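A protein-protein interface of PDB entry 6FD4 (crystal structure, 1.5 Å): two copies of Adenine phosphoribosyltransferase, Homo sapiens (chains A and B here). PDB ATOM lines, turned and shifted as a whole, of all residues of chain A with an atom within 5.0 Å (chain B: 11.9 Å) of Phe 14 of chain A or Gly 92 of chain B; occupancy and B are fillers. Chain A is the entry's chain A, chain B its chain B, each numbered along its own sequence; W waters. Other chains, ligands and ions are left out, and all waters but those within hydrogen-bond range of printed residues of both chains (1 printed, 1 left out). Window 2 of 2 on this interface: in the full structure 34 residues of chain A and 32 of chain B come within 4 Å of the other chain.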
ATOM      1  N   ARG A  12     -28.179  26.900  14.967  1.00  0.00           N
ATOM      2  CA  ARG A  12     -27.645  26.189  13.836  1.00  0.00           C
ATOM      3  C   ARG A  12     -27.690  24.702  14.220  1.00  0.00           C
ATOM      4  O   ARG A  12     -27.227  24.330  15.277  1.00  0.00           O
ATOM      5  CB  ARG A  12     -26.194  26.649  13.583  1.00  0.00           C
ATOM      6  CG  ARG A  12     -25.476  25.955  12.453  1.00  0.00           C
ATOM      7  CD  ARG A  12     -24.192  26.686  12.076  1.00  0.00           C
ATOM      8  NE  ARG A  12     -23.372  26.970  13.245  1.00  0.00           N
ATOM      9  CZ  ARG A  12     -22.069  27.215  13.214  1.00  0.00           C
ATOM     10  NH1 ARG A  12     -21.419  27.204  12.060  1.00  0.00           N
ATOM     11  NH2 ARG A  12     -21.415  27.478  14.342  1.00  0.00           N
ATOM     12  N   SER A  13     -28.343  23.886  13.405  1.00  0.00           N
ATOM     13  CA  SER A  13     -28.598  22.495  13.763  1.00  0.00           C
ATOM     14  C   SER A  13     -27.671  21.553  13.017  1.00  0.00           C
ATOM     15  O   SER A  13     -27.648  21.563  11.787  1.00  0.00           O
ATOM     16  CB  SER A  13     -30.060  22.139  13.453  1.00  0.00           C
ATOM     17  OG  SER A  13     -30.938  22.842  14.313  1.00  0.00           O
ATOM     18  N   PHE A  14     -26.865  20.782  13.759  1.00  0.00           N
ATOM     19  CA  PHE A  14     -25.903  19.845  13.180  1.00  0.00           C
ATOM     20  C   PHE A  14     -26.378  18.413  13.348  1.00  0.00           C
ATOM     21  O   PHE A  14     -26.522  17.925  14.476  1.00  0.00           O
ATOM     22  CB  PHE A  14     -24.548  19.951  13.888  1.00  0.00           C
ATOM     23  CG  PHE A  14     -23.775  21.172  13.536  1.00  0.00           C
ATOM     24  CD1 PHE A  14     -23.999  22.362  14.216  1.00  0.00           C
ATOM     25  CD2 PHE A  14     -22.837  21.142  12.501  1.00  0.00           C
ATOM     26  CE1 PHE A  14     -23.283  23.500  13.888  1.00  0.00           C
ATOM     27  CE2 PHE A  14     -22.119  22.288  12.171  1.00  0.00           C
ATOM     28  CZ  PHE A  14     -22.337  23.453  12.869  1.00  0.00           C
ATOM     29  N   PRO A  15     -26.625  17.724  12.236  1.00  0.00           N
ATOM     30  CA  PRO A  15     -27.067  16.333  12.334  1.00  0.00           C
ATOM     31  C   PRO A  15     -25.950  15.392  12.747  1.00  0.00           C
ATOM     32  O   PRO A  15     -24.782  15.647  12.448  1.00  0.00           O
ATOM     33  CB  PRO A  15     -27.519  16.006  10.913  1.00  0.00           C
ATOM     34  CG  PRO A  15     -26.746  16.934  10.048  1.00  0.00           C
ATOM     35  CD  PRO A  15     -26.476  18.172  10.843  1.00  0.00           C
ATOM     36  N   ASP A  16     -26.296  14.319  13.453  1.00  0.00           N
ATOM     37  CA  ASP A  16     -25.339  13.270  13.787  1.00  0.00           C
ATOM     38  C   ASP A  16     -24.157  13.747  14.629  1.00  0.00           C
ATOM     39  O   ASP A  16     -23.050  13.239  14.510  1.00  0.00           O
ATOM     40  CB  ASP A  16     -24.831  12.605  12.523  1.00  0.00           C
ATOM     41  CG  ASP A  16     -25.948  12.156  11.647  1.00  0.00           C
ATOM     42  OD1 ASP A  16     -26.866  11.478  12.167  1.00  0.00           O
ATOM     43  OD2 ASP A  16     -25.925  12.477  10.442  1.00  0.00           O
ATOM     44  N   PHE A  17     -24.432  14.672  15.533  1.00  0.00           N
ATOM     45  CA  PHE A  17     -23.451  15.102  16.526  1.00  0.00           C
ATOM     46  C   PHE A  17     -24.155  15.153  17.883  1.00  0.00           C
ATOM     47  O   PHE A  17     -25.211  15.776  18.020  1.00  0.00           O
ATOM     48  CB  PHE A  17     -22.866  16.477  16.178  1.00  0.00           C
ATOM     49  CG  PHE A  17     -21.789  16.909  17.124  1.00  0.00           C
ATOM     50  CD1 PHE A  17     -20.469  16.548  16.887  1.00  0.00           C
ATOM     51  CD2 PHE A  17     -22.096  17.615  18.276  1.00  0.00           C
ATOM     52  CE1 PHE A  17     -19.473  16.905  17.779  1.00  0.00           C
ATOM     53  CE2 PHE A  17     -21.104  17.965  19.178  1.00  0.00           C
ATOM     54  CZ  PHE A  17     -19.790  17.605  18.926  1.00  0.00           C
ATOM     55  N   VAL A  22     -28.832  11.972  16.246  1.00  0.00           N
ATOM     56  CA  VAL A  22     -29.102  13.105  17.110  1.00  0.00           C
ATOM     57  C   VAL A  22     -28.747  14.402  16.408  1.00  0.00           C
ATOM     58  O   VAL A  22     -27.724  14.473  15.731  1.00  0.00           O
ATOM     59  CB  VAL A  22     -28.237  13.011  18.374  1.00  0.00           C
ATOM     60  CG1 VAL A  22     -28.628  14.076  19.375  1.00  0.00           C
ATOM     61  CG2 VAL A  22     -28.389  11.633  18.994  1.00  0.00           C
ATOM     62  N   VAL A  23     -29.578  15.414  16.590  1.00  0.00           N
ATOM     63  CA  VAL A  23     -29.294  16.731  16.067  1.00  0.00           C
ATOM     64  C   VAL A  23     -28.851  17.653  17.196  1.00  0.00           C
ATOM     65  O   VAL A  23     -29.526  17.771  18.210  1.00  0.00           O
ATOM     66  CB  VAL A  23     -30.532  17.329  15.376  1.00  0.00           C
ATOM     67  CG1 VAL A  23     -30.231  18.728  14.872  1.00  0.00           C
ATOM     68  CG2 VAL A  23     -31.001  16.427  14.248  1.00  0.00           C
ATOM     69  N   PHE A  24     -27.705  18.291  17.003  1.00  0.00           N
ATOM     70  CA  PHE A  24     -27.125  19.211  17.971  1.00  0.00           C
ATOM     71  C   PHE A  24     -27.590  20.619  17.657  1.00  0.00           C
ATOM     72  O   PHE A  24     -27.419  21.079  16.539  1.00  0.00           O
ATOM     73  CB  PHE A  24     -25.606  19.152  17.882  1.00  0.00           C
ATOM     74  CG  PHE A  24     -24.904  19.933  18.944  1.00  0.00           C
ATOM     75  CD1 PHE A  24     -24.567  21.251  18.743  1.00  0.00           C
ATOM     76  CD2 PHE A  24     -24.564  19.326  20.134  1.00  0.00           C
ATOM     77  CE1 PHE A  24     -23.900  21.962  19.719  1.00  0.00           C
ATOM     78  CE2 PHE A  24     -23.901  20.037  21.121  1.00  0.00           C
ATOM     79  CZ  PHE A  24     -23.576  21.352  20.909  1.00  0.00           C
ATOM     80  N   ASP A  26     -26.830  24.181  18.010  1.00  0.00           N
ATOM     81  CA  ASP A  26     -25.674  25.032  18.295  1.00  0.00           C
ATOM     82  C   ASP A  26     -26.157  26.468  18.542  1.00  0.00           C
ATOM     83  O   ASP A  26     -26.752  27.101  17.664  1.00  0.00           O
ATOM     84  CB  ASP A  26     -24.698  24.969  17.113  1.00  0.00           C
ATOM     85  CG  ASP A  26     -23.445  25.822  17.314  1.00  0.00           C
ATOM     86  OD1 ASP A  26     -23.136  26.170  18.470  1.00  0.00           O
ATOM     87  OD2 ASP A  26     -22.795  26.131  16.289  1.00  0.00           O
ATOM     88  N   LEU B  83     -16.818  31.624  20.901  1.00  0.00           N
ATOM     89  CA  LEU B  83     -16.486  30.665  21.931  1.00  0.00           C
ATOM     90  C   LEU B  83     -15.239  29.872  21.573  1.00  0.00           C
ATOM     91  O   LEU B  83     -15.119  29.361  20.450  1.00  0.00           O
ATOM     92  CB  LEU B  83     -17.623  29.655  22.108  1.00  0.00           C
ATOM     93  CG  LEU B  83     -19.006  30.246  22.353  1.00  0.00           C
ATOM     94  CD1 LEU B  83     -20.034  29.146  22.584  1.00  0.00           C
ATOM     95  CD2 LEU B  83     -18.981  31.180  23.549  1.00  0.00           C
ATOM     96  N   ARG B  85     -13.619  26.467  23.267  1.00  0.00           N
ATOM     97  CA  ARG B  85     -14.068  25.446  24.212  1.00  0.00           C
ATOM     98  C   ARG B  85     -12.996  24.436  24.538  1.00  0.00           C
ATOM     99  O   ARG B  85     -12.061  24.228  23.756  1.00  0.00           O
ATOM    100  CB  ARG B  85     -15.277  24.717  23.624  1.00  0.00           C
ATOM    101  CG  ARG B  85     -16.506  25.589  23.502  1.00  0.00           C
ATOM    102  CD  ARG B  85     -17.758  24.873  23.998  1.00  0.00           C
ATOM    103  NE  ARG B  85     -17.597  24.457  25.386  1.00  0.00           N
ATOM    104  CZ  ARG B  85     -18.492  23.765  26.088  1.00  0.00           C
ATOM    105  NH1 ARG B  85     -19.649  23.393  25.536  1.00  0.00           N
ATOM    106  NH2 ARG B  85     -18.215  23.441  27.347  1.00  0.00           N
ATOM    107  N   LYS B  86     -13.147  23.734  25.657  1.00  0.00           N
ATOM    108  CA  LYS B  86     -12.404  22.500  25.864  1.00  0.00           C
ATOM    109  C   LYS B  86     -12.745  21.510  24.752  1.00  0.00           C
ATOM    110  O   LYS B  86     -13.875  21.421  24.298  1.00  0.00           O
ATOM    111  CB  LYS B  86     -12.710  21.932  27.236  1.00  0.00           C
ATOM    112  CG  LYS B  86     -12.374  22.878  28.366  1.00  0.00           C
ATOM    113  CD  LYS B  86     -10.887  23.096  28.502  1.00  0.00           C
ATOM    114  CE  LYS B  86     -10.571  24.229  29.459  1.00  0.00           C
ATOM    115  NZ  LYS B  86     -10.765  23.819  30.874  1.00  0.00           N
ATOM    116  N   ARG B  87     -11.732  20.810  24.251  1.00  0.00           N
ATOM    117  CA  ARG B  87     -11.946  19.928  23.123  1.00  0.00           C
ATOM    118  C   ARG B  87     -13.039  18.883  23.361  1.00  0.00           C
ATOM    119  O   ARG B  87     -13.147  18.308  24.442  1.00  0.00           O
ATOM    120  CB  ARG B  87     -10.641  19.215  22.757  1.00  0.00           C
ATOM    121  CG  ARG B  87     -10.796  18.415  21.477  1.00  0.00           C
ATOM    122  CD  ARG B  87      -9.487  17.832  21.011  1.00  0.00           C
ATOM    123  NE  ARG B  87      -9.714  16.921  19.897  1.00  0.00           N
ATOM    124  CZ  ARG B  87      -8.794  16.077  19.451  1.00  0.00           C
ATOM    125  NH1 ARG B  87      -9.064  15.259  18.441  1.00  0.00           N
ATOM    126  NH2 ARG B  87      -7.611  16.063  20.041  1.00  0.00           N
ATOM    127  N   GLY B  88     -13.822  18.633  22.314  1.00  0.00           N
ATOM    128  CA  GLY B  88     -14.832  17.585  22.331  1.00  0.00           C
ATOM    129  C   GLY B  88     -16.266  18.065  22.401  1.00  0.00           C
ATOM    130  O   GLY B  88     -17.185  17.244  22.399  1.00  0.00           O
ATOM    131  N   LYS B  89     -16.476  19.372  22.440  1.00  0.00           N
ATOM    132  CA  LYS B  89     -17.788  19.918  22.736  1.00  0.00           C
ATOM    133  C   LYS B  89     -18.447  20.614  21.552  1.00  0.00           C
ATOM    134  O   LYS B  89     -19.649  20.894  21.577  1.00  0.00           O
ATOM    135  CB  LYS B  89     -17.658  20.926  23.872  1.00  0.00           C
ATOM    136  CG  LYS B  89     -17.106  20.351  25.175  1.00  0.00           C
ATOM    137  CD  LYS B  89     -17.909  19.147  25.632  1.00  0.00           C
ATOM    138  CE  LYS B  89     -19.317  19.531  26.062  1.00  0.00           C
ATOM    139  NZ  LYS B  89     -20.082  18.365  26.577  1.00  0.00           N
ATOM    140  N   LEU B  90     -17.649  20.992  20.565  1.00  0.00           N
ATOM    141  CA  LEU B  90     -18.140  21.812  19.467  1.00  0.00           C
ATOM    142  C   LEU B  90     -18.433  20.950  18.258  1.00  0.00           C
ATOM    143  O   LEU B  90     -17.651  20.056  17.939  1.00  0.00           O
ATOM    144  CB  LEU B  90     -17.083  22.822  19.076  1.00  0.00           C
ATOM    145  CG  LEU B  90     -16.900  23.977  20.051  1.00  0.00           C
ATOM    146  CD1 LEU B  90     -15.638  24.754  19.723  1.00  0.00           C
ATOM    147  CD2 LEU B  90     -18.111  24.875  20.047  1.00  0.00           C
ATOM    148  N   PRO B  91     -19.567  21.216  17.575  1.00  0.00           N
ATOM    149  CA  PRO B  91     -19.917  20.565  16.333  1.00  0.00           C
ATOM    150  C   PRO B  91     -19.214  21.195  15.137  1.00  0.00           C
ATOM    151  O   PRO B  91     -18.680  22.304  15.252  1.00  0.00           O
ATOM    152  CB  PRO B  91     -21.419  20.822  16.252  1.00  0.00           C
ATOM    153  CG  PRO B  91     -21.574  22.168  16.831  1.00  0.00           C
ATOM    154  CD  PRO B  91     -20.602  22.195  17.981  1.00  0.00           C
ATOM    155  N   GLY B  92     -19.229  20.497  14.008  1.00  0.00           N
ATOM    156  CA  GLY B  92     -18.620  21.013  12.775  1.00  0.00           C
ATOM    157  C   GLY B  92     -17.110  20.915  12.758  1.00  0.00           C
ATOM    158  O   GLY B  92     -16.481  20.466  13.713  1.00  0.00           O
ATOM    159  N   PRO B  93     -16.502  21.343  11.654  1.00  0.00           N
ATOM    160  CA  PRO B  93     -15.051  21.288  11.554  1.00  0.00           C
ATOM    161  C   PRO B  93     -14.373  22.162  12.598  1.00  0.00           C
ATOM    162  O   PRO B  93     -14.795  23.295  12.804  1.00  0.00           O
ATOM    163  CB  PRO B  93     -14.781  21.833  10.149  1.00  0.00           C
ATOM    164  CG  PRO B  93     -16.040  21.586   9.396  1.00  0.00           C
ATOM    165  CD  PRO B  93     -17.127  21.777  10.394  1.00  0.00           C
ATOM    166  N   THR B  94     -13.326  21.643  13.223  1.00  0.00           N
ATOM    167  CA  THR B  94     -12.620  22.368  14.285  1.00  0.00           C
ATOM    168  C   THR B  94     -11.100  22.277  14.152  1.00  0.00           C
ATOM    169  O   THR B  94     -10.569  21.471  13.372  1.00  0.00           O
ATOM    170  CB  THR B  94     -12.960  21.840  15.672  1.00  0.00           C
ATOM    171  OG1 THR B  94     -12.447  20.505  15.789  1.00  0.00           O
ATOM    172  CG2 THR B  94     -14.466  21.884  15.918  1.00  0.00           C
ATOM    173  N   LEU B  95     -10.428  23.174  14.877  1.00  0.00           N
ATOM    174  CA  LEU B  95      -8.991  23.148  15.112  1.00  0.00           C
ATOM    175  C   LEU B  95      -8.819  23.082  16.611  1.00  0.00           C
ATOM    176  O   LEU B  95      -9.656  23.608  17.355  1.00  0.00           O
ATOM    177  CB  LEU B  95      -8.313  24.438  14.641  1.00  0.00           C
ATOM    178  CG  LEU B  95      -8.677  25.052  13.299  1.00  0.00           C
ATOM    179  CD1 LEU B  95      -7.901  26.347  13.073  1.00  0.00           C
ATOM    180  CD2 LEU B  95      -8.348  24.023  12.231  1.00  0.00           C
ATOM    181  N   TRP B  96      -7.725  22.502  17.061  1.00  0.00           N
ATOM    182  CA  TRP B  96      -7.465  22.397  18.487  1.00  0.00           C
ATOM    183  C   TRP B  96      -5.992  22.638  18.798  1.00  0.00           C
ATOM    184  O   TRP B  96      -5.119  22.552  17.929  1.00  0.00           O
ATOM    185  CB  TRP B  96      -7.968  21.053  19.057  1.00  0.00           C
ATOM    186  CG  TRP B  96      -7.370  19.841  18.460  1.00  0.00           C
ATOM    187  CD1 TRP B  96      -6.212  19.242  18.817  1.00  0.00           C
ATOM    188  CD2 TRP B  96      -7.912  19.062  17.385  1.00  0.00           C
ATOM    189  NE1 TRP B  96      -5.981  18.142  18.021  1.00  0.00           N
ATOM    190  CE2 TRP B  96      -7.015  18.001  17.143  1.00  0.00           C
ATOM    191  CE3 TRP B  96      -9.069  19.152  16.612  1.00  0.00           C
ATOM    192  CZ2 TRP B  96      -7.235  17.045  16.145  1.00  0.00           C
ATOM    193  CZ3 TRP B  96      -9.297  18.199  15.652  1.00  0.00           C
ATOM    194  CH2 TRP B  96      -8.381  17.151  15.434  1.00  0.00           C
ATOM    195  N   LEU B 108      -7.757  23.139  23.938  1.00  0.00           N
ATOM    196  CA  LEU B 108      -8.826  24.027  23.543  1.00  0.00           C
ATOM    197  C   LEU B 108      -9.154  23.809  22.071  1.00  0.00           C
ATOM    198  O   LEU B 108      -8.320  23.285  21.325  1.00  0.00           O
ATOM    199  CB  LEU B 108      -8.439  25.488  23.723  1.00  0.00           C
ATOM    200  CG  LEU B 108      -8.171  25.961  25.140  1.00  0.00           C
ATOM    201  CD1 LEU B 108      -7.950  27.469  25.174  1.00  0.00           C
ATOM    202  CD2 LEU B 108      -9.305  25.577  26.066  1.00  0.00           C
ATOM    203  N   GLU B 109     -10.340  24.238  21.676  1.00  0.00           N
ATOM    204  CA  GLU B 109     -10.863  23.992  20.332  1.00  0.00           C
ATOM    205  C   GLU B 109     -11.716  25.166  19.863  1.00  0.00           C
ATOM    206  O   GLU B 109     -12.381  25.836  20.655  1.00  0.00           O
ATOM    207  CB  GLU B 109     -11.687  22.698  20.369  1.00  0.00           C
ATOM    208  CG  GLU B 109     -12.174  22.167  19.041  1.00  0.00           C
ATOM    209  CD  GLU B 109     -12.725  20.757  19.145  1.00  0.00           C
ATOM    210  OE1 GLU B 109     -12.397  19.933  18.274  1.00  0.00           O
ATOM    211  OE2 GLU B 109     -13.470  20.471  20.098  1.00  0.00           O
ATOM    212  N   ILE B 110     -11.708  25.420  18.561  1.00  0.00           N
ATOM    213  CA  ILE B 110     -12.499  26.486  17.986  1.00  0.00           C
ATOM    214  C   ILE B 110     -13.055  25.978  16.669  1.00  0.00           C
ATOM    215  O   ILE B 110     -12.408  25.161  15.995  1.00  0.00           O
ATOM    216  CB  ILE B 110     -11.648  27.744  17.769  1.00  0.00           C
ATOM    217  CG1 ILE B 110     -12.523  28.964  17.508  1.00  0.00           C
ATOM    218  CG2 ILE B 110     -10.643  27.521  16.653  1.00  0.00           C
ATOM    219  CD1 ILE B 110     -11.777  30.280  17.602  1.00  0.00           C
ATOM    220  N   GLN B 111     -14.267  26.385  16.324  1.00  0.00           N
ATOM    221  CA  GLN B 111     -14.825  26.044  14.993  1.00  0.00           C
ATOM    222  C   GLN B 111     -14.025  26.748  13.897  1.00  0.00           C
ATOM    223  O   GLN B 111     -13.646  27.909  14.045  1.00  0.00           O
ATOM    224  CB  GLN B 111     -16.311  26.399  14.909  1.00  0.00           C
ATOM    225  CG  GLN B 111     -17.171  25.556  15.846  1.00  0.00           C
ATOM    226  CD  GLN B 111     -18.630  25.989  15.923  1.00  0.00           C
ATOM    227  OE1 GLN B 111     -18.959  27.184  15.941  1.00  0.00           O
ATOM    228  NE2 GLN B 111     -19.512  25.018  15.946  1.00  0.00           N
ATOM    229  N   LYS B 112     -13.789  26.050  12.782  1.00  0.00           N
ATOM    230  CA  LYS B 112     -13.014  26.634  11.671  1.00  0.00           C
ATOM    231  C   LYS B 112     -13.675  27.889  11.104  1.00  0.00           C
ATOM    232  O   LYS B 112     -12.976  28.746  10.585  1.00  0.00           O
ATOM    233  CB  LYS B 112     -12.787  25.630  10.549  1.00  0.00           C
ATOM    234  CG  LYS B 112     -11.899  24.454  10.895  1.00  0.00           C
ATOM    235  CD  LYS B 112     -11.489  23.718   9.633  1.00  0.00           C
ATOM    236  CE  LYS B 112     -10.756  22.440   9.930  1.00  0.00           C
ATOM    237  NZ  LYS B 112     -10.370  21.723   8.684  1.00  0.00           N
ATOM    238  N   ASP B 113     -15.003  28.002  11.223  1.00  0.00           N
ATOM    239  CA  ASP B 113     -15.712  29.181  10.734  1.00  0.00           C
ATOM    240  C   ASP B 113     -16.045  30.204  11.815  1.00  0.00           C
ATOM    241  O   ASP B 113     -16.874  31.098  11.592  1.00  0.00           O
ATOM    242  CB  ASP B 113     -16.971  28.773   9.952  1.00  0.00           C
ATOM    243  CG  ASP B 113     -18.040  28.149  10.821  1.00  0.00           C
ATOM    244  OD1 ASP B 113     -17.879  28.075  12.051  1.00  0.00           O
ATOM    245  OD2 ASP B 113     -19.064  27.720  10.248  1.00  0.00           O
ATOM    246  N   ALA B 114     -15.349  30.164  12.952  1.00  0.00           N
ATOM    247  CA  ALA B 114     -15.637  31.111  14.033  1.00  0.00           C
ATOM    248  C   ALA B 114     -15.315  32.566  13.658  1.00  0.00           C
ATOM    249  O   ALA B 114     -16.002  33.502  14.099  1.00  0.00           O
ATOM    250  CB  ALA B 114     -14.887  30.722  15.288  1.00  0.00           C
ATOM    251  N   LEU B 144      -6.681  30.820  12.441  1.00  0.00           N
ATOM    252  CA  LEU B 144      -7.782  31.320  11.642  1.00  0.00           C
ATOM    253  C   LEU B 144      -7.450  32.630  10.930  1.00  0.00           C
ATOM    254  O   LEU B 144      -8.321  33.208  10.268  1.00  0.00           O
ATOM    255  CB  LEU B 144      -9.033  31.537  12.491  1.00  0.00           C
ATOM    256  CG  LEU B 144      -9.647  30.275  13.100  1.00  0.00           C
ATOM    257  CD1 LEU B 144     -10.878  30.645  13.923  1.00  0.00           C
ATOM    258  CD2 LEU B 144      -9.991  29.269  12.022  1.00  0.00           C
HETATM  259  O   HOH W   1     -18.692  29.443  14.209  1.00  0.00           O
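The side-chain amide oxygen (OE1) of Gln 111 of chain B sits at hydrogen-bond distance from the guanidinium group (NH2) of Arg 12 of chain A.
NE2 of Gln 111 of chain B sits at hydrogen-bond distance from OD2 of Asp 26 of chain A.
OD2 of Asp 113 of chain B lies within salt-bridge range of NH1 of Arg 12 of chain A (3.0 Å).
The backbone carbonyl oxygen (O) of Pro 91 of chain B sits at hydrogen-bond distance from the side-chain amide nitrogen (NE2) of Gln 111 of chain B, at 2.9 Å.
The guanidinium group of Arg 12 of chain A lies within salt-bridge range of the side-chain carboxylate of Asp 26 of chain A (2.7 Å).
The backbone carbonyl oxygen (O) of Phe 14 of chain A sits at hydrogen-bond distance from the backbone NH (N) of Phe 24 of chain A, 2.8 Å away.
N of Phe 17 of chain A is in hydrogen-bond range of O of Val 22 of chain A (3.3 Å).
Among the printed residues, pairs that only touch across the chains: Phe 17 of chain A with Leu 90 of chain B, Phe 14 of chain A with Pro 91 of chain B, Phe 24 of chain A with Pro 91 of chain B, Phe 14 of chain A with Gly 92 of chain B and Phe 17 of chain A with Pro 91 of chain B.
Of chain B, only Pro 91 (3.6 Å) and Gly 92 (3.8 Å) come within 4 Å of Phe 14 of chain A.
No residue of chain B comes within 4 Å of Asp 16 of chain A.
Printed residues of chain B within 4 Å of Phe 17 of chain A: Leu 90 and Pro 91.
No residue of chain B comes within 4 Å of Val 23 of chain A.
Of the printed residues of chain B, Phe 24 of chain A touches Pro 91.
Lys 86 of chain B touches none of the printed residues of chain A.
Of the printed residues of chain A, Leu 90 of chain B touches Phe 17.
Printed residues of chain A within 4 Å of Pro 91 of chain B: Phe 14 (3.6 Å), Phe 17 (3.9 Å) and Phe 24 (3.7 Å).
Gly 92 of chain B touches just one residue of chain A: Phe 14.
Printed residues of chain A within 4 Å of Gln 111 of chain B: Arg 12 and Asp 26.
Of the printed residues of chain A, Asp 113 of chain B touches Arg 12 (3.0 Å).
Ala 114 of chain B touches none of the printed residues of chain A.
The nearest residue of chain B that does not touch Phe 14 of chain A is Gln 111 of chain B (4.5 Å).
The nearest printed residue of chain A that does not touch Gly 92 of chain B is Phe 17 of chain A (5.0 Å).
The nearest printed residue of chain A that does not touch Gln 111 of chain B is Phe 14 of chain A (4.5 Å).
Hydrophobic or aromatic side chains of chain B within 4 Å of the printed part of chain A: Pro 91.
Among the printed residues, 8 pairs touch across the chains.
No position is printed for both chains.
Of the 8 pairs that touch across the chains among the printed residues, none has its exchanged pair printed and touching as well.
Water W1 lies within hydrogen-bond range of the side-chain carboxylate of Asp 113 of chain B (2.7 Å), the side-chain amide oxygen of Gln 111 of chain B (2.9 Å) and the guanidinium group of Arg 12 of chain A (3.4 Å).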
